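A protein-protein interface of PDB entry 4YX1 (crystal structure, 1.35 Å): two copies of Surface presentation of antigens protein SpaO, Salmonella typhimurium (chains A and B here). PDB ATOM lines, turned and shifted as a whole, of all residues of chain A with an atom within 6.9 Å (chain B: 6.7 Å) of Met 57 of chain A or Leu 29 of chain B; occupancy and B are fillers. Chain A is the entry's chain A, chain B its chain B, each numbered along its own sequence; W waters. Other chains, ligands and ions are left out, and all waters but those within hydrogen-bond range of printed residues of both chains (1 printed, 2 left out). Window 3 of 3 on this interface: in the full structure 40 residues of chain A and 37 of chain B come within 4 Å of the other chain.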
ATOM      1  N   GLU A  53      27.096  18.938 -25.963  1.00  0.00           N
ATOM      2  CA  GLU A  53      26.346  18.062 -25.099  1.00  0.00           C
ATOM      3  C   GLU A  53      26.123  18.751 -23.782  1.00  0.00           C
ATOM      4  O   GLU A  53      27.029  19.375 -23.249  1.00  0.00           O
ATOM      5  CB  GLU A  53      27.115  16.761 -24.928  1.00  0.00           C
ATOM      6  CG  GLU A  53      26.528  15.792 -23.945  1.00  0.00           C
ATOM      7  CD  GLU A  53      27.297  14.493 -23.909  1.00  0.00           C
ATOM      8  OE1 GLU A  53      28.251  14.319 -24.691  1.00  0.00           O
ATOM      9  OE2 GLU A  53      26.943  13.630 -23.099  1.00  0.00           O
ATOM     10  N   VAL A  55      25.919  19.212 -19.947  1.00  0.00           N
ATOM     11  CA  VAL A  55      26.651  18.626 -18.820  1.00  0.00           C
ATOM     12  C   VAL A  55      26.229  19.329 -17.543  1.00  0.00           C
ATOM     13  O   VAL A  55      26.038  20.541 -17.541  1.00  0.00           O
ATOM     14  CB  VAL A  55      28.180  18.773 -19.005  1.00  0.00           C
ATOM     15  CG1 VAL A  55      28.951  18.370 -17.745  1.00  0.00           C
ATOM     16  CG2 VAL A  55      28.646  17.975 -20.213  1.00  0.00           C
ATOM     17  N   GLN A  56      26.057  18.580 -16.462  1.00  0.00           N
ATOM     18  CA  GLN A  56      25.871  19.214 -15.163  1.00  0.00           C
ATOM     19  C   GLN A  56      27.229  19.457 -14.543  1.00  0.00           C
ATOM     20  O   GLN A  56      27.962  18.512 -14.248  1.00  0.00           O
ATOM     21  CB  GLN A  56      25.024  18.355 -14.228  1.00  0.00           C
ATOM     22  CG  GLN A  56      24.970  18.917 -12.811  1.00  0.00           C
ATOM     23  CD  GLN A  56      24.123  20.157 -12.711  1.00  0.00           C
ATOM     24  OE1 GLN A  56      22.897  20.098 -12.830  1.00  0.00           O
ATOM     25  NE2 GLN A  56      24.767  21.293 -12.500  1.00  0.00           N
ATOM     26  N   MET A  57      27.577  20.727 -14.385  1.00  0.00           N
ATOM     27  CA  MET A  57      28.843  21.122 -13.782  1.00  0.00           C
ATOM     28  C   MET A  57      28.612  21.348 -12.292  1.00  0.00           C
ATOM     29  O   MET A  57      27.525  21.064 -11.779  1.00  0.00           O
ATOM     30  CB  MET A  57      29.390  22.378 -14.467  1.00  0.00           C
ATOM     31  CG  MET A  57      29.517  22.247 -15.982  1.00  0.00           C
ATOM     32  SD  MET A  57      30.207  23.855 -16.824  1.00  0.00           S
ATOM     33  CE  MET A  57      31.979  23.877 -16.021  1.00  0.00           C
ATOM     34  N   ASN A  58      29.611  21.845 -11.574  1.00  0.00           N
ATOM     35  CA  ASN A  58      29.444  21.972 -10.124  1.00  0.00           C
ATOM     36  C   ASN A  58      28.407  23.002  -9.690  1.00  0.00           C
ATOM     37  O   ASN A  58      27.691  22.786  -8.709  1.00  0.00           O
ATOM     38  CB  ASN A  58      30.789  22.288  -9.470  1.00  0.00           C
ATOM     39  CG  ASN A  58      31.698  21.077  -9.428  1.00  0.00           C
ATOM     40  OD1 ASN A  58      31.228  19.955  -9.276  1.00  0.00           O
ATOM     41  ND2 ASN A  58      32.998  21.296  -9.564  1.00  0.00           N
ATOM     42  N   ASP A  59      28.312  24.116 -10.406  1.00  0.00           N
ATOM     43  CA  ASP A  59      27.429  25.185  -9.967  1.00  0.00           C
ATOM     44  C   ASP A  59      26.406  25.569 -11.023  1.00  0.00           C
ATOM     45  O   ASP A  59      25.464  26.306 -10.745  1.00  0.00           O
ATOM     46  CB  ASP A  59      28.256  26.409  -9.563  1.00  0.00           C
ATOM     47  CG  ASP A  59      29.004  26.199  -8.258  1.00  0.00           C
ATOM     48  OD1 ASP A  59      28.423  25.618  -7.313  1.00  0.00           O
ATOM     49  OD2 ASP A  59      30.186  26.599  -8.179  1.00  0.00           O
ATOM     50  N   THR A  60      26.593  25.073 -12.241  1.00  0.00           N
ATOM     51  CA  THR A  60      25.716  25.422 -13.355  1.00  0.00           C
ATOM     52  C   THR A  60      25.608  24.265 -14.330  1.00  0.00           C
ATOM     53  O   THR A  60      26.283  23.253 -14.184  1.00  0.00           O
ATOM     54  CB  THR A  60      26.231  26.650 -14.150  1.00  0.00           C
ATOM     55  OG1 THR A  60      27.490  26.322 -14.758  1.00  0.00           O
ATOM     56  CG2 THR A  60      26.386  27.897 -13.268  1.00  0.00           C
ATOM     57  N   LEU A  61      24.777  24.430 -15.348  1.00  0.00           N
ATOM     58  CA  LEU A  61      24.860  23.560 -16.510  1.00  0.00           C
ATOM     59  C   LEU A  61      25.968  24.058 -17.411  1.00  0.00           C
ATOM     60  O   LEU A  61      26.347  25.228 -17.360  1.00  0.00           O
ATOM     61  CB  LEU A  61      23.545  23.515 -17.286  1.00  0.00           C
ATOM     62  CG  LEU A  61      22.363  22.903 -16.534  1.00  0.00           C
ATOM     63  CD1 LEU A  61      21.172  22.831 -17.462  1.00  0.00           C
ATOM     64  CD2 LEU A  61      22.710  21.521 -15.982  1.00  0.00           C
ATOM     65  N   GLY A  62      26.491  23.167 -18.238  1.00  0.00           N
ATOM     66  CA  GLY A  62      27.473  23.558 -19.216  1.00  0.00           C
ATOM     67  C   GLY A  62      27.193  22.883 -20.537  1.00  0.00           C
ATOM     68  O   GLY A  62      26.375  21.974 -20.623  1.00  0.00           O
ATOM     69  N   VAL A  63      27.890  23.334 -21.572  1.00  0.00           N
ATOM     70  CA  VAL A  63      27.827  22.674 -22.864  1.00  0.00           C
ATOM     71  C   VAL A  63      29.230  22.224 -23.239  1.00  0.00           C
ATOM     72  O   VAL A  63      30.135  23.039 -23.411  1.00  0.00           O
ATOM     73  CB  VAL A  63      27.238  23.584 -23.958  1.00  0.00           C
ATOM     74  CG1 VAL A  63      27.253  22.864 -25.300  1.00  0.00           C
ATOM     75  CG2 VAL A  63      25.825  24.000 -23.579  1.00  0.00           C
ATOM     76  N   GLU A  64      29.406  20.909 -23.323  1.00  0.00           N
ATOM     77  CA  GLU A  64      30.648  20.312 -23.776  1.00  0.00           C
ATOM     78  C   GLU A  64      30.673  20.333 -25.296  1.00  0.00           C
ATOM     79  O   GLU A  64      29.865  19.667 -25.927  1.00  0.00           O
ATOM     80  CB  GLU A  64      30.756  18.882 -23.249  1.00  0.00           C
ATOM     81  CG  GLU A  64      32.004  18.153 -23.724  1.00  0.00           C
ATOM     82  CD  GLU A  64      31.950  16.669 -23.435  1.00  0.00           C
ATOM     83  OE1 GLU A  64      30.880  16.181 -23.010  1.00  0.00           O
ATOM     84  OE2 GLU A  64      32.969  15.988 -23.643  1.00  0.00           O
ATOM     85  N   ILE A  65      31.582  21.096 -25.890  1.00  0.00           N
ATOM     86  CA  ILE A  65      31.583  21.241 -27.348  1.00  0.00           C
ATOM     87  C   ILE A  65      32.056  19.950 -28.020  1.00  0.00           C
ATOM     88  O   ILE A  65      33.078  19.372 -27.643  1.00  0.00           O
ATOM     89  CB  ILE A  65      32.480  22.412 -27.800  1.00  0.00           C
ATOM     90  CG1 ILE A  65      32.054  23.718 -27.121  1.00  0.00           C
ATOM     91  CG2 ILE A  65      32.483  22.553 -29.333  1.00  0.00           C
ATOM     92  CD1 ILE A  65      30.678  24.155 -27.478  1.00  0.00           C
ATOM     93  N   GLN B  27      36.904  27.783 -26.650  1.00  0.00           N
ATOM     94  CA  GLN B  27      36.579  27.001 -25.465  1.00  0.00           C
ATOM     95  C   GLN B  27      36.049  25.620 -25.824  1.00  0.00           C
ATOM     96  O   GLN B  27      35.423  25.430 -26.875  1.00  0.00           O
ATOM     97  CB  GLN B  27      35.555  27.745 -24.604  1.00  0.00           C
ATOM     98  CG  GLN B  27      35.973  29.160 -24.212  1.00  0.00           C
ATOM     99  CD  GLN B  27      37.081  29.169 -23.179  1.00  0.00           C
ATOM    100  OE1 GLN B  27      37.179  28.256 -22.359  1.00  0.00           O
ATOM    101  NE2 GLN B  27      37.929  30.195 -23.216  1.00  0.00           N
ATOM    102  N   GLN B  28      36.289  24.652 -24.945  1.00  0.00           N
ATOM    103  CA  GLN B  28      35.742  23.311 -25.151  1.00  0.00           C
ATOM    104  C   GLN B  28      34.572  22.975 -24.214  1.00  0.00           C
ATOM    105  O   GLN B  28      33.803  22.064 -24.488  1.00  0.00           O
ATOM    106  CB  GLN B  28      36.847  22.257 -25.019  1.00  0.00           C
ATOM    107  CG  GLN B  28      37.651  22.117 -26.312  1.00  0.00           C
ATOM    108  CD  GLN B  28      36.781  21.708 -27.509  1.00  0.00           C
ATOM    109  OE1 GLN B  28      36.060  20.714 -27.465  1.00  0.00           O
ATOM    110  NE2 GLN B  28      36.812  22.519 -28.570  1.00  0.00           N
ATOM    111  N   LEU B  29      34.429  23.716 -23.121  1.00  0.00           N
ATOM    112  CA  LEU B  29      33.325  23.512 -22.190  1.00  0.00           C
ATOM    113  C   LEU B  29      32.805  24.887 -21.783  1.00  0.00           C
ATOM    114  O   LEU B  29      33.530  25.677 -21.179  1.00  0.00           O
ATOM    115  CB  LEU B  29      33.779  22.694 -20.977  1.00  0.00           C
ATOM    116  CG  LEU B  29      32.758  22.462 -19.856  1.00  0.00           C
ATOM    117  CD1 LEU B  29      31.518  21.750 -20.367  1.00  0.00           C
ATOM    118  CD2 LEU B  29      33.367  21.678 -18.693  1.00  0.00           C
ATOM    119  N   LEU B  30      31.561  25.179 -22.151  1.00  0.00           N
ATOM    120  CA  LEU B  30      30.969  26.490 -21.918  1.00  0.00           C
ATOM    121  C   LEU B  30      30.033  26.454 -20.730  1.00  0.00           C
ATOM    122  O   LEU B  30      29.129  25.635 -20.691  1.00  0.00           O
ATOM    123  CB  LEU B  30      30.203  26.960 -23.154  1.00  0.00           C
ATOM    124  CG  LEU B  30      31.017  27.199 -24.423  1.00  0.00           C
ATOM    125  CD1 LEU B  30      30.082  27.578 -25.570  1.00  0.00           C
ATOM    126  CD2 LEU B  30      32.023  28.295 -24.159  1.00  0.00           C
ATOM    127  N   SER B  31      30.241  27.341 -19.766  1.00  0.00           N
ATOM    128  CA  SER B  31      29.335  27.428 -18.636  1.00  0.00           C
ATOM    129  C   SER B  31      28.125  28.290 -18.981  1.00  0.00           C
ATOM    130  O   SER B  31      28.261  29.370 -19.546  1.00  0.00           O
ATOM    131  CB  SER B  31      30.059  27.994 -17.412  1.00  0.00           C
ATOM    132  OG  SER B  31      31.135  27.158 -17.022  1.00  0.00           O
ATOM    133  N   LEU B  32      26.939  27.805 -18.639  1.00  0.00           N
ATOM    134  CA  LEU B  32      25.730  28.609 -18.748  1.00  0.00           C
ATOM    135  C   LEU B  32      25.485  29.302 -17.419  1.00  0.00           C
ATOM    136  O   LEU B  32      25.997  28.869 -16.389  1.00  0.00           O
ATOM    137  CB  LEU B  32      24.533  27.741 -19.137  1.00  0.00           C
ATOM    138  CG  LEU B  32      24.725  27.005 -20.461  1.00  0.00           C
ATOM    139  CD1 LEU B  32      23.517  26.160 -20.771  1.00  0.00           C
ATOM    140  CD2 LEU B  32      25.003  27.988 -21.590  1.00  0.00           C
HETATM  141  O   HOH W   1      30.110  26.610 -14.288  1.00  0.00           O
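Of the printed residues of chain A, Gln 28 of chain B touches Val 63, Glu 64 and Ile 65.
Of the printed residues of chain B, Gly 62 of chain A touches Leu 30 (3.0 Å).
Of the printed residues of chain A, Ser 31 of chain B touches Met 57 and Leu 61.
Glu 53 of chain A touches none of the printed residues of chain B.
Asp 59 of chain A touches none of the printed residues of chain B.
The nearest residue of chain B that does not touch Met 57 of chain A is Leu 30 of chain B (4.4 Å).
The nearest residue of chain A that does not touch Leu 29 of chain B is Gly 62 of chain A (4.5 Å).
Water W1 lies within hydrogen-bond range of the side-chain hydroxyl of Thr 60 of chain A, the side-chain hydroxyl of Ser 31 of chain B and the side-chain sulfur of Met 57 of chain A.
Printed residues of chain A that touch a printed residue of chain B: Met 57, Thr 60, Leu 61, Gly 62, Val 63, Glu 64 and Ile 65.
Hydrophobic or aromatic side chains of chain A that line the printed part of chain B: Met 57 and Ile 65.
Printed residues of chain B that touch a printed residue of chain A: Gln 27, Gln 28, Leu 29, Leu 30, Ser 31 and Leu 32.
The backbone carbonyl oxygen of Val 55 of chain A sits at hydrogen-bond distance from the backbone NH of Gly 62 of chain A (2.8 Å).
NE2 of Gln 56 of chain A lies within hydrogen-bond range of O of Thr 60 of chain A, at 3.0 Å.
The backbone carbonyl oxygen (O) of Glu 53 of chain A sits at hydrogen-bond distance from the backbone NH (N) of Glu 64 of chain A (2.8 Å).
Among the printed residues, merely in contact across the chains: Gly 62 of chain A with Leu 30 of chain B, Val 63 of chain A with Leu 29 of chain B, Glu 64 of chain A with Gln 28 of chain B, Met 57 of chain A with Leu 29 of chain B, Glu 64 of chain A with Leu 29 of chain B, Ile 65 of chain A with Gln 27 of chain B, Leu 61 of chain A with Ser 31 of chain B, Val 63 of chain A with Gln 28 of chain B and Ile 65 of chain A with Leu 30 of chain B.
N of Val 63 of chain A is in hydrogen-bond range of O of Leu 30 of chain B (2.8 Å).
The side-chain hydroxyl (OG) of Ser 31 of chain B lies within hydrogen-bond range of the side-chain sulfur (SD) of Met 57 of chain A (3.4 Å).
OG1 of Thr 60 of chain A lies close to O of Leu 32 of chain B (3.4 Å).
The backbone NH of Leu 32 of chain B lies within hydrogen-bond range of the backbone carbonyl oxygen of Leu 61 of chain A, at 2.9 Å.
N of Ile 65 of chain A lies within hydrogen-bond range of O of Gln 28 of chain B, at 2.8 Å.
No position is printed for both chains.
Of the 14 pairs that touch across the chains among the printed residues, none has its exchanged pair printed and touching as well.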
